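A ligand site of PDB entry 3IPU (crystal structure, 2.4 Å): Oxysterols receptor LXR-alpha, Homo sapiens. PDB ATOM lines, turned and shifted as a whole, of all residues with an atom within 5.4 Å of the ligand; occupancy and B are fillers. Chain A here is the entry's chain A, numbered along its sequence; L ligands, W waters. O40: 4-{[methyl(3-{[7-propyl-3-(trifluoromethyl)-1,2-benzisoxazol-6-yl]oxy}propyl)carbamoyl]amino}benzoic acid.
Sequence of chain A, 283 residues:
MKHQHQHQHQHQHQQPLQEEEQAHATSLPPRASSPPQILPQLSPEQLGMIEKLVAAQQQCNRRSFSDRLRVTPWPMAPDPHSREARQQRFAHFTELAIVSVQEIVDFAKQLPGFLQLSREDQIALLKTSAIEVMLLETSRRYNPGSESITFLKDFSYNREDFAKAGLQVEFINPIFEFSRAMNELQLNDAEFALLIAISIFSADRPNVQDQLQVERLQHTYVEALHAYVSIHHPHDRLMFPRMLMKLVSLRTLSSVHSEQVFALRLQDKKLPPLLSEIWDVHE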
ATOM      1  N   ASN A  61      -8.443 -11.537 -11.927  1.00  0.00           N
ATOM      2  CA  ASN A  61      -9.467 -11.998 -10.962  1.00  0.00           C
ATOM      3  C   ASN A  61      -9.777 -13.499 -11.031  1.00  0.00           C
ATOM      4  O   ASN A  61      -9.942 -14.143  -9.987  1.00  0.00           O
ATOM      5  CB  ASN A  61     -10.762 -11.197 -11.148  1.00  0.00           C
ATOM      6  CG  ASN A  61     -11.881 -11.685 -10.224  1.00  0.00           C
ATOM      7  OD1 ASN A  61     -11.999 -11.238  -9.068  1.00  0.00           O
ATOM      8  ND2 ASN A  61     -12.721 -12.579 -10.747  1.00  0.00           N
ATOM      9  N   ARG A  68      -8.998 -17.521  -3.445  1.00  0.00           N
ATOM     10  CA  ARG A  68     -10.098 -16.812  -2.777  1.00  0.00           C
ATOM     11  C   ARG A  68     -11.148 -17.768  -2.210  1.00  0.00           C
ATOM     12  O   ARG A  68     -11.904 -17.413  -1.297  1.00  0.00           O
ATOM     13  CB  ARG A  68     -10.748 -15.847  -3.775  1.00  0.00           C
ATOM     14  CG  ARG A  68     -11.751 -14.873  -3.191  1.00  0.00           C
ATOM     15  CD  ARG A  68     -11.922 -13.691  -4.144  1.00  0.00           C
ATOM     16  NE  ARG A  68     -10.842 -12.723  -4.004  1.00  0.00           N
ATOM     17  CZ  ARG A  68     -10.457 -11.857  -4.951  1.00  0.00           C
ATOM     18  NH1 ARG A  68     -11.034 -11.841  -6.146  1.00  0.00           N
ATOM     19  NH2 ARG A  68      -9.470 -11.017  -4.684  1.00  0.00           N
ATOM     20  N   PHE A  90     -10.864 -11.532  11.538  1.00  0.00           N
ATOM     21  CA  PHE A  90      -9.618 -10.874  11.225  1.00  0.00           C
ATOM     22  C   PHE A  90      -8.828 -11.700  10.220  1.00  0.00           C
ATOM     23  O   PHE A  90      -8.284 -11.145   9.255  1.00  0.00           O
ATOM     24  CB  PHE A  90      -8.790 -10.660  12.486  1.00  0.00           C
ATOM     25  CG  PHE A  90      -7.465  -9.985  12.240  1.00  0.00           C
ATOM     26  CD1 PHE A  90      -7.407  -8.622  11.995  1.00  0.00           C
ATOM     27  CD2 PHE A  90      -6.283 -10.727  12.232  1.00  0.00           C
ATOM     28  CE1 PHE A  90      -6.187  -7.995  11.773  1.00  0.00           C
ATOM     29  CE2 PHE A  90      -5.057 -10.114  12.004  1.00  0.00           C
ATOM     30  CZ  PHE A  90      -5.014  -8.752  11.779  1.00  0.00           C
ATOM     31  N   PHE A  93     -10.599 -11.290   6.780  1.00  0.00           N
ATOM     32  CA  PHE A  93     -10.372  -9.989   6.137  1.00  0.00           C
ATOM     33  C   PHE A  93      -8.948  -9.822   5.604  1.00  0.00           C
ATOM     34  O   PHE A  93      -8.754  -9.367   4.483  1.00  0.00           O
ATOM     35  CB  PHE A  93     -10.743  -8.832   7.089  1.00  0.00           C
ATOM     36  CG  PHE A  93     -11.944  -8.047   6.636  1.00  0.00           C
ATOM     37  CD1 PHE A  93     -13.198  -8.647   6.598  1.00  0.00           C
ATOM     38  CD2 PHE A  93     -11.810  -6.723   6.231  1.00  0.00           C
ATOM     39  CE1 PHE A  93     -14.317  -7.948   6.170  1.00  0.00           C
ATOM     40  CE2 PHE A  93     -12.926  -6.002   5.801  1.00  0.00           C
ATOM     41  CZ  PHE A  93     -14.189  -6.609   5.771  1.00  0.00           C
ATOM     42  N   THR A  94      -7.964 -10.201   6.417  1.00  0.00           N
ATOM     43  CA  THR A  94      -6.570 -10.111   6.016  1.00  0.00           C
ATOM     44  C   THR A  94      -6.255 -11.032   4.833  1.00  0.00           C
ATOM     45  O   THR A  94      -5.390 -10.722   3.999  1.00  0.00           O
ATOM     46  CB  THR A  94      -5.618 -10.421   7.186  1.00  0.00           C
ATOM     47  OG1 THR A  94      -5.969 -11.667   7.792  1.00  0.00           O
ATOM     48  CG2 THR A  94      -5.656  -9.288   8.212  1.00  0.00           C
ATOM     49  N   LEU A  96      -8.505 -11.840   2.496  1.00  0.00           N
ATOM     50  CA  LEU A  96      -9.029 -11.101   1.347  1.00  0.00           C
ATOM     51  C   LEU A  96      -7.983 -10.116   0.814  1.00  0.00           C
ATOM     52  O   LEU A  96      -7.795  -9.983  -0.393  1.00  0.00           O
ATOM     53  CB  LEU A  96     -10.329 -10.352   1.710  1.00  0.00           C
ATOM     54  CG  LEU A  96     -11.572 -11.195   2.017  1.00  0.00           C
ATOM     55  CD1 LEU A  96     -12.762 -10.286   2.351  1.00  0.00           C
ATOM     56  CD2 LEU A  96     -11.911 -12.142   0.880  1.00  0.00           C
ATOM     57  N   ALA A  97      -7.291  -9.433   1.734  1.00  0.00           N
ATOM     58  CA  ALA A  97      -6.276  -8.440   1.384  1.00  0.00           C
ATOM     59  C   ALA A  97      -5.039  -9.074   0.736  1.00  0.00           C
ATOM     60  O   ALA A  97      -4.468  -8.522  -0.215  1.00  0.00           O
ATOM     61  CB  ALA A  97      -5.892  -7.642   2.621  1.00  0.00           C
ATOM     62  N   SER A 100      -5.953  -9.818  -2.814  1.00  0.00           N
ATOM     63  CA  SER A 100      -6.037  -8.541  -3.477  1.00  0.00           C
ATOM     64  C   SER A 100      -4.640  -8.052  -3.921  1.00  0.00           C
ATOM     65  O   SER A 100      -4.459  -7.684  -5.074  1.00  0.00           O
ATOM     66  CB  SER A 100      -6.725  -7.520  -2.541  1.00  0.00           C
ATOM     67  OG  SER A 100      -7.041  -6.310  -3.223  1.00  0.00           O
ATOM     68  N   GLU A 103      -3.520  -9.962  -6.925  1.00  0.00           N
ATOM     69  CA  GLU A 103      -4.157  -9.362  -8.092  1.00  0.00           C
ATOM     70  C   GLU A 103      -3.551  -8.032  -8.501  1.00  0.00           C
ATOM     71  O   GLU A 103      -3.402  -7.749  -9.703  1.00  0.00           O
ATOM     72  CB  GLU A 103      -5.657  -9.149  -7.815  1.00  0.00           C
ATOM     73  CG  GLU A 103      -6.426 -10.460  -7.751  1.00  0.00           C
ATOM     74  CD  GLU A 103      -7.882 -10.276  -7.429  1.00  0.00           C
ATOM     75  OE1 GLU A 103      -8.281  -9.150  -7.052  1.00  0.00           O
ATOM     76  OE2 GLU A 103      -8.620 -11.277  -7.530  1.00  0.00           O
ATOM     77  N   ILE A 131      -2.460  -0.226  -0.815  1.00  0.00           N
ATOM     78  CA  ILE A 131      -3.622   0.161   0.001  1.00  0.00           C
ATOM     79  C   ILE A 131      -4.558   1.052  -0.778  1.00  0.00           C
ATOM     80  O   ILE A 131      -5.779   0.929  -0.658  1.00  0.00           O
ATOM     81  CB  ILE A 131      -3.232   0.837   1.368  1.00  0.00           C
ATOM     82  CG1 ILE A 131      -4.505   1.099   2.194  1.00  0.00           C
ATOM     83  CG2 ILE A 131      -2.387   2.101   1.173  1.00  0.00           C
ATOM     84  CD1 ILE A 131      -5.316  -0.184   2.519  1.00  0.00           C
ATOM     85  N   MET A 134      -6.452  -1.087  -3.258  1.00  0.00           N
ATOM     86  CA  MET A 134      -7.443  -1.827  -2.470  1.00  0.00           C
ATOM     87  C   MET A 134      -8.655  -0.977  -2.054  1.00  0.00           C
ATOM     88  O   MET A 134      -9.791  -1.467  -2.047  1.00  0.00           O
ATOM     89  CB  MET A 134      -6.810  -2.388  -1.212  1.00  0.00           C
ATOM     90  CG  MET A 134      -6.407  -3.827  -1.265  1.00  0.00           C
ATOM     91  SD  MET A 134      -5.555  -4.233   0.300  1.00  0.00           S
ATOM     92  CE  MET A 134      -3.892  -3.897  -0.237  1.00  0.00           C
ATOM     93  N   LEU A 135      -8.401   0.266  -1.640  1.00  0.00           N
ATOM     94  CA  LEU A 135      -9.472   1.193  -1.282  1.00  0.00           C
ATOM     95  C   LEU A 135     -10.332   1.532  -2.510  1.00  0.00           C
ATOM     96  O   LEU A 135     -11.557   1.607  -2.426  1.00  0.00           O
ATOM     97  CB  LEU A 135      -8.917   2.455  -0.606  1.00  0.00           C
ATOM     98  CG  LEU A 135      -8.419   2.263   0.835  1.00  0.00           C
ATOM     99  CD1 LEU A 135      -7.481   3.365   1.271  1.00  0.00           C
ATOM    100  CD2 LEU A 135      -9.563   2.163   1.821  1.00  0.00           C
ATOM    101  N   GLU A 137     -10.758  -0.501  -5.162  1.00  0.00           N
ATOM    102  CA  GLU A 137     -11.551  -1.721  -5.410  1.00  0.00           C
ATOM    103  C   GLU A 137     -12.663  -1.888  -4.400  1.00  0.00           C
ATOM    104  O   GLU A 137     -13.736  -2.386  -4.724  1.00  0.00           O
ATOM    105  CB  GLU A 137     -10.668  -2.977  -5.312  1.00  0.00           C
ATOM    106  CG  GLU A 137      -9.653  -3.194  -6.431  1.00  0.00           C
ATOM    107  CD  GLU A 137     -10.278  -3.464  -7.788  1.00  0.00           C
ATOM    108  OE1 GLU A 137     -11.517  -3.433  -7.906  1.00  0.00           O
ATOM    109  OE2 GLU A 137      -9.519  -3.695  -8.747  1.00  0.00           O
ATOM    110  N   THR A 138     -12.405  -1.502  -3.156  1.00  0.00           N
ATOM    111  CA  THR A 138     -13.436  -1.461  -2.127  1.00  0.00           C
ATOM    112  C   THR A 138     -14.597  -0.533  -2.531  1.00  0.00           C
ATOM    113  O   THR A 138     -15.747  -0.924  -2.426  1.00  0.00           O
ATOM    114  CB  THR A 138     -12.844  -1.023  -0.753  1.00  0.00           C
ATOM    115  OG1 THR A 138     -11.916  -2.015  -0.282  1.00  0.00           O
ATOM    116  CG2 THR A 138     -13.952  -0.817   0.291  1.00  0.00           C
ATOM    117  N   ARG A 141     -17.125  -1.754  -5.077  1.00  0.00           N
ATOM    118  CA  ARG A 141     -18.042  -2.807  -4.637  1.00  0.00           C
ATOM    119  C   ARG A 141     -19.012  -2.319  -3.569  1.00  0.00           C
ATOM    120  O   ARG A 141     -19.587  -3.102  -2.831  1.00  0.00           O
ATOM    121  CB  ARG A 141     -17.222  -3.970  -4.095  1.00  0.00           C
ATOM    122  CG  ARG A 141     -16.343  -4.572  -5.157  1.00  0.00           C
ATOM    123  CD  ARG A 141     -15.354  -5.586  -4.627  1.00  0.00           C
ATOM    124  NE  ARG A 141     -14.937  -6.457  -5.725  1.00  0.00           N
ATOM    125  CZ  ARG A 141     -14.146  -6.086  -6.732  1.00  0.00           C
ATOM    126  NH1 ARG A 141     -13.652  -4.853  -6.814  1.00  0.00           N
ATOM    127  NH2 ARG A 141     -13.841  -6.955  -7.694  1.00  0.00           N
ATOM    128  N   PHE A 151     -17.691  -7.934  -0.882  1.00  0.00           N
ATOM    129  CA  PHE A 151     -16.485  -8.642  -1.289  1.00  0.00           C
ATOM    130  C   PHE A 151     -16.884  -9.993  -1.910  1.00  0.00           C
ATOM    131  O   PHE A 151     -17.005 -10.080  -3.139  1.00  0.00           O
ATOM    132  CB  PHE A 151     -15.531  -8.779  -0.095  1.00  0.00           C
ATOM    133  CG  PHE A 151     -15.006  -7.452   0.410  1.00  0.00           C
ATOM    134  CD1 PHE A 151     -14.457  -6.517  -0.465  1.00  0.00           C
ATOM    135  CD2 PHE A 151     -15.054  -7.146   1.762  1.00  0.00           C
ATOM    136  CE1 PHE A 151     -13.965  -5.297  -0.008  1.00  0.00           C
ATOM    137  CE2 PHE A 151     -14.565  -5.924   2.244  1.00  0.00           C
ATOM    138  CZ  PHE A 151     -14.022  -4.998   1.352  1.00  0.00           C
ATOM    139  N   LEU A 152     -17.117 -11.020  -1.100  1.00  0.00           N
ATOM    140  CA  LEU A 152     -17.597 -12.310  -1.645  1.00  0.00           C
ATOM    141  C   LEU A 152     -19.070 -12.169  -2.043  1.00  0.00           C
ATOM    142  O   LEU A 152     -19.807 -11.417  -1.426  1.00  0.00           O
ATOM    143  CB  LEU A 152     -17.411 -13.458  -0.632  1.00  0.00           C
ATOM    144  CG  LEU A 152     -16.096 -14.256  -0.753  1.00  0.00           C
ATOM    145  CD1 LEU A 152     -16.165 -15.219  -1.939  1.00  0.00           C
ATOM    146  CD2 LEU A 152     -14.867 -13.371  -0.879  1.00  0.00           C
ATOM    147  N   LYS A 153     -19.471 -12.933  -3.071  1.00  0.00           N
ATOM    148  CA  LYS A 153     -20.640 -12.586  -3.907  1.00  0.00           C
ATOM    149  C   LYS A 153     -21.984 -12.501  -3.170  1.00  0.00           C
ATOM    150  O   LYS A 153     -22.732 -11.521  -3.344  1.00  0.00           O
ATOM    151  CB  LYS A 153     -20.767 -13.562  -5.071  1.00  0.00           C
ATOM    152  CG  LYS A 153     -21.534 -12.994  -6.286  1.00  0.00           C
ATOM    153  CD  LYS A 153     -20.851 -13.332  -7.620  1.00  0.00           C
ATOM    154  CE  LYS A 153     -19.505 -12.586  -7.780  1.00  0.00           C
ATOM    155  NZ  LYS A 153     -18.934 -12.672  -9.145  1.00  0.00           N
ATOM    156  N   PHE A 162     -16.756  -4.497   9.651  1.00  0.00           N
ATOM    157  CA  PHE A 162     -15.360  -4.039   9.607  1.00  0.00           C
ATOM    158  C   PHE A 162     -14.779  -3.942  11.007  1.00  0.00           C
ATOM    159  O   PHE A 162     -13.645  -4.380  11.244  1.00  0.00           O
ATOM    160  CB  PHE A 162     -15.243  -2.672   8.926  1.00  0.00           C
ATOM    161  CG  PHE A 162     -15.128  -2.732   7.416  1.00  0.00           C
ATOM    162  CD1 PHE A 162     -16.141  -3.285   6.653  1.00  0.00           C
ATOM    163  CD2 PHE A 162     -14.019  -2.183   6.770  1.00  0.00           C
ATOM    164  CE1 PHE A 162     -16.048  -3.330   5.255  1.00  0.00           C
ATOM    165  CE2 PHE A 162     -13.909  -2.219   5.385  1.00  0.00           C
ATOM    166  CZ  PHE A 162     -14.925  -2.795   4.624  1.00  0.00           C
ATOM    167  N   LEU A 167     -10.838  -3.759  12.551  1.00  0.00           N
ATOM    168  CA  LEU A 167     -10.488  -2.411  12.110  1.00  0.00           C
ATOM    169  C   LEU A 167     -11.076  -1.370  13.076  1.00  0.00           C
ATOM    170  O   LEU A 167     -12.143  -1.560  13.623  1.00  0.00           O
ATOM    171  CB  LEU A 167     -10.960  -2.187  10.664  1.00  0.00           C
ATOM    172  CG  LEU A 167     -10.134  -2.876   9.552  1.00  0.00           C
ATOM    173  CD1 LEU A 167     -10.210  -4.430   9.617  1.00  0.00           C
ATOM    174  CD2 LEU A 167     -10.555  -2.396   8.172  1.00  0.00           C
ATOM    175  N   PHE A 171     -10.638   4.500  10.965  1.00  0.00           N
ATOM    176  CA  PHE A 171     -10.284   4.073   9.619  1.00  0.00           C
ATOM    177  C   PHE A 171     -11.525   3.666   8.849  1.00  0.00           C
ATOM    178  O   PHE A 171     -11.691   4.046   7.683  1.00  0.00           O
ATOM    179  CB  PHE A 171      -9.272   2.915   9.677  1.00  0.00           C
ATOM    180  CG  PHE A 171      -8.730   2.474   8.354  1.00  0.00           C
ATOM    181  CD1 PHE A 171      -8.488   3.389   7.319  1.00  0.00           C
ATOM    182  CD2 PHE A 171      -8.432   1.137   8.141  1.00  0.00           C
ATOM    183  CE1 PHE A 171      -7.972   2.967   6.095  1.00  0.00           C
ATOM    184  CE2 PHE A 171      -7.922   0.713   6.934  1.00  0.00           C
ATOM    185  CZ  PHE A 171      -7.685   1.634   5.910  1.00  0.00           C
ATOM    186  N   ILE A 175     -13.292   5.093   5.162  1.00  0.00           N
ATOM    187  CA  ILE A 175     -13.367   4.163   4.034  1.00  0.00           C
ATOM    188  C   ILE A 175     -14.756   4.282   3.402  1.00  0.00           C
ATOM    189  O   ILE A 175     -14.888   4.442   2.186  1.00  0.00           O
ATOM    190  CB  ILE A 175     -13.127   2.688   4.469  1.00  0.00           C
ATOM    191  CG1 ILE A 175     -11.685   2.454   4.909  1.00  0.00           C
ATOM    192  CG2 ILE A 175     -13.477   1.712   3.342  1.00  0.00           C
ATOM    193  CD1 ILE A 175     -11.490   1.112   5.671  1.00  0.00           C
ATOM    194  N   HIS A 257      -4.747   4.849   7.214  1.00  0.00           N
ATOM    195  CA  HIS A 257      -4.397   3.441   7.180  1.00  0.00           C
ATOM    196  C   HIS A 257      -3.098   3.124   7.915  1.00  0.00           C
ATOM    197  O   HIS A 257      -3.013   2.106   8.591  1.00  0.00           O
ATOM    198  CB  HIS A 257      -4.301   2.933   5.748  1.00  0.00           C
ATOM    199  CG  HIS A 257      -3.764   1.538   5.660  1.00  0.00           C
ATOM    200  ND1 HIS A 257      -2.447   1.282   5.341  1.00  0.00           N
ATOM    201  CD2 HIS A 257      -4.342   0.344   5.880  1.00  0.00           C
ATOM    202  CE1 HIS A 257      -2.251  -0.031   5.346  1.00  0.00           C
ATOM    203  NE2 HIS A 257      -3.382  -0.617   5.677  1.00  0.00           N
ATOM    204  N   GLN A 260      -3.842   2.889  11.391  1.00  0.00           N
ATOM    205  CA  GLN A 260      -4.500   1.612  11.632  1.00  0.00           C
ATOM    206  C   GLN A 260      -3.480   0.488  11.877  1.00  0.00           C
ATOM    207  O   GLN A 260      -3.635  -0.301  12.802  1.00  0.00           O
ATOM    208  CB  GLN A 260      -5.417   1.266  10.449  1.00  0.00           C
ATOM    209  CG  GLN A 260      -5.988  -0.154  10.486  1.00  0.00           C
ATOM    210  CD  GLN A 260      -7.002  -0.340  11.599  1.00  0.00           C
ATOM    211  OE1 GLN A 260      -8.161   0.059  11.458  1.00  0.00           O
ATOM    212  NE2 GLN A 260      -6.579  -0.957  12.687  1.00  0.00           N
ATOM    213  N   VAL A 261      -2.443   0.442  11.046  1.00  0.00           N
ATOM    214  CA  VAL A 261      -1.398  -0.573  11.133  1.00  0.00           C
ATOM    215  C   VAL A 261      -0.608  -0.420  12.432  1.00  0.00           C
ATOM    216  O   VAL A 261      -0.164  -1.413  13.021  1.00  0.00           O
ATOM    217  CB  VAL A 261      -0.460  -0.476   9.906  1.00  0.00           C
ATOM    218  CG1 VAL A 261       0.856  -1.265  10.113  1.00  0.00           C
ATOM    219  CG2 VAL A 261      -1.192  -0.950   8.664  1.00  0.00           C
ATOM    220  N   LEU A 264      -2.638  -1.860  15.414  1.00  0.00           N
ATOM    221  CA  LEU A 264      -2.579  -3.331  15.434  1.00  0.00           C
ATOM    222  C   LEU A 264      -1.424  -3.798  16.282  1.00  0.00           C
ATOM    223  O   LEU A 264      -1.557  -4.720  17.087  1.00  0.00           O
ATOM    224  CB  LEU A 264      -2.440  -3.902  14.031  1.00  0.00           C
ATOM    225  CG  LEU A 264      -3.718  -4.319  13.308  1.00  0.00           C
ATOM    226  CD1 LEU A 264      -4.898  -3.570  13.828  1.00  0.00           C
ATOM    227  CD2 LEU A 264      -3.539  -4.119  11.807  1.00  0.00           C
ATOM    228  N   LEU A 271      -0.035  -8.914  11.575  1.00  0.00           N
ATOM    229  CA  LEU A 271      -0.444  -9.033  10.184  1.00  0.00           C
ATOM    230  C   LEU A 271       0.194 -10.268   9.590  1.00  0.00           C
ATOM    231  O   LEU A 271       1.319 -10.647   9.957  1.00  0.00           O
ATOM    232  CB  LEU A 271      -0.049  -7.793   9.377  1.00  0.00           C
ATOM    233  CG  LEU A 271      -0.894  -6.534   9.532  1.00  0.00           C
ATOM    234  CD1 LEU A 271      -0.178  -5.370   8.873  1.00  0.00           C
ATOM    235  CD2 LEU A 271      -2.284  -6.715   8.935  1.00  0.00           C
ATOM    236  N   LEU A 275       1.196  -8.869   4.118  1.00  0.00           N
ATOM    237  CA  LEU A 275       0.722  -7.572   4.604  1.00  0.00           C
ATOM    238  C   LEU A 275       1.749  -6.949   5.555  1.00  0.00           C
ATOM    239  O   LEU A 275       1.992  -5.746   5.504  1.00  0.00           O
ATOM    240  CB  LEU A 275      -0.652  -7.691   5.284  1.00  0.00           C
ATOM    241  CG  LEU A 275      -1.806  -8.366   4.541  1.00  0.00           C
ATOM    242  CD1 LEU A 275      -3.085  -8.248   5.353  1.00  0.00           C
ATOM    243  CD2 LEU A 275      -2.002  -7.795   3.120  1.00  0.00           C
ATOM    244  N   TRP A 279       3.338  -3.385   4.833  1.00  0.00           N
ATOM    245  CA  TRP A 279       2.705  -2.364   5.682  1.00  0.00           C
ATOM    246  C   TRP A 279       3.365  -2.056   7.002  1.00  0.00           C
ATOM    247  O   TRP A 279       3.287  -0.916   7.462  1.00  0.00           O
ATOM    248  CB  TRP A 279       1.233  -2.700   5.912  1.00  0.00           C
ATOM    249  CG  TRP A 279       0.401  -2.557   4.698  1.00  0.00           C
ATOM    250  CD1 TRP A 279       0.654  -1.779   3.600  1.00  0.00           C
ATOM    251  CD2 TRP A 279      -0.867  -3.167   4.475  1.00  0.00           C
ATOM    252  NE1 TRP A 279      -0.366  -1.907   2.697  1.00  0.00           N
ATOM    253  CE2 TRP A 279      -1.318  -2.747   3.216  1.00  0.00           C
ATOM    254  CE3 TRP A 279      -1.679  -4.037   5.220  1.00  0.00           C
ATOM    255  CZ2 TRP A 279      -2.532  -3.147   2.665  1.00  0.00           C
ATOM    256  CZ3 TRP A 279      -2.889  -4.441   4.682  1.00  0.00           C
ATOM    257  CH2 TRP A 279      -3.309  -4.004   3.412  1.00  0.00           C
HETATM  258  C1  O40 L   1      -8.336  -6.093   4.780  1.00  0.00           C
HETATM  259  C2  O40 L   1      -8.547  -5.111   3.798  1.00  0.00           C
HETATM  260  C3  O40 L   1      -7.986  -3.816   3.910  1.00  0.00           C
HETATM  261  C4  O40 L   1      -7.201  -3.574   5.038  1.00  0.00           C
HETATM  262  C5  O40 L   1      -7.017  -4.568   5.978  1.00  0.00           C
HETATM  263  C6  O40 L   1      -7.555  -5.838   5.890  1.00  0.00           C
HETATM  264  O7  O40 L   1      -6.537  -2.377   5.357  1.00  0.00           O
HETATM  265  N8  O40 L   1      -5.873  -2.644   6.607  1.00  0.00           N
HETATM  266  C9  O40 L   1      -6.160  -3.849   6.951  1.00  0.00           C
HETATM  267  C10 O40 L   1     -13.162  -9.480  -2.887  1.00  0.00           C
HETATM  268  O11 O40 L   1      -9.331  -5.388   2.689  1.00  0.00           O
HETATM  269  C12 O40 L   1      -8.202  -2.720   2.866  1.00  0.00           C
HETATM  270  C13 O40 L   1     -13.854 -10.506  -3.537  1.00  0.00           C
HETATM  271  C14 O40 L   1      -5.660  -4.573   8.151  1.00  0.00           C
HETATM  272  C15 O40 L   1     -10.092  -6.607   2.586  1.00  0.00           C
HETATM  273  C16 O40 L   1     -13.833 -10.600  -4.936  1.00  0.00           C
HETATM  274  C17 O40 L   1      -9.391  -1.794   3.252  1.00  0.00           C
HETATM  275  C18 O40 L   1     -13.104  -9.660  -5.672  1.00  0.00           C
HETATM  276  C19 O40 L   1     -12.402  -8.653  -5.015  1.00  0.00           C
HETATM  277  C20 O40 L   1     -10.752  -2.540   3.309  1.00  0.00           C
HETATM  278  N21 O40 L   1     -10.532  -6.451  -1.253  1.00  0.00           N
HETATM  279  C22 O40 L   1     -10.518  -5.169  -1.976  1.00  0.00           C
HETATM  280  C23 O40 L   1     -11.148  -7.539  -1.816  1.00  0.00           C
HETATM  281  N24 O40 L   1     -11.739  -7.516  -2.996  1.00  0.00           N
HETATM  282  C26 O40 L   1     -10.849  -6.528   1.251  1.00  0.00           C
HETATM  283  C29 O40 L   1      -9.853  -6.549   0.054  1.00  0.00           C
HETATM  284  O30 O40 L   1     -15.163 -12.670  -4.882  1.00  0.00           O
HETATM  285  C32 O40 L   1     -14.591 -11.716  -5.642  1.00  0.00           C
HETATM  286  O33 O40 L   1     -11.152  -8.581  -1.198  1.00  0.00           O
HETATM  287  O34 O40 L   1     -14.693 -11.696  -6.866  1.00  0.00           O
HETATM  288  F38 O40 L   1      -4.855  -3.716   8.859  1.00  0.00           F
HETATM  289  F39 O40 L   1      -4.939  -5.618   7.646  1.00  0.00           F
HETATM  290  F40 O40 L   1      -6.637  -5.126   8.925  1.00  0.00           F
HETATM  291  C42 O40 L   1     -12.420  -8.537  -3.618  1.00  0.00           C
HETATM  292  O   HOH W   1     -10.721  -6.180  -4.863  1.00  0.00           O
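NH1 of Arg 68 is in salt-bridge range of O34 of the ligand (3.7 Å).
A nitrogen (N8) of the ligand sits at hydrogen-bond distance from a ring nitrogen (NE2) of His 257 (3.3 Å).
Residues that only touch the ligand: Asn 61 (3.5 Å), Phe 93 (3.3 Å), Thr 94 (3.8 Å), Leu 96 (3.5 Å), Ala 97 (3.6 Å), Ser 100 (3.9 Å), Ile 131 (3.8 Å), Met 134 (3.8 Å), Glu 137 (3.99 Å), Thr 138 (3.8 Å), Arg 141 (3.4 Å), Phe 151 (3.2 Å), Phe 162 (3.8 Å), Leu 167 (3.7 Å), Phe 171 (3.7 Å), Leu 264 (3.3 Å), Leu 271 (3.1 Å), Leu 275 (3.95 Å) and Trp 279 (3.8 Å).
Hydrophobic or aromatic side chains within 4 Å of the ligand: Phe 93, Leu 96, Ala 97, Ile 131, Met 134, Phe 151, Phe 162, Leu 167, Phe 171, His 257, Leu 264, Leu 271, Leu 275 and Trp 279.
The nearest printed residue that does not touch the ligand is Leu 152 (4.02 Å).
The side-chain amide oxygen of Asn 61 sits at hydrogen-bond distance from the guanidinium group of Arg 68.
O of Met 134 lies within hydrogen-bond range of OG1 of Thr 138 (2.8 Å).
NH1 of Arg 141 lies within salt-bridge range of OE1 of Glu 137.
The backbone carbonyl oxygen (O) of Phe 162 is in hydrogen-bond range of the backbone NH (N) of Leu 167 (3.2 Å).
The guanidinium group (NH1) of Arg 68 is in salt-bridge range of the side-chain carboxylate (OE2) of Glu 103, 2.8 Å away.
O of Phe 90 is in hydrogen-bond range of OG1 of Thr 94.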
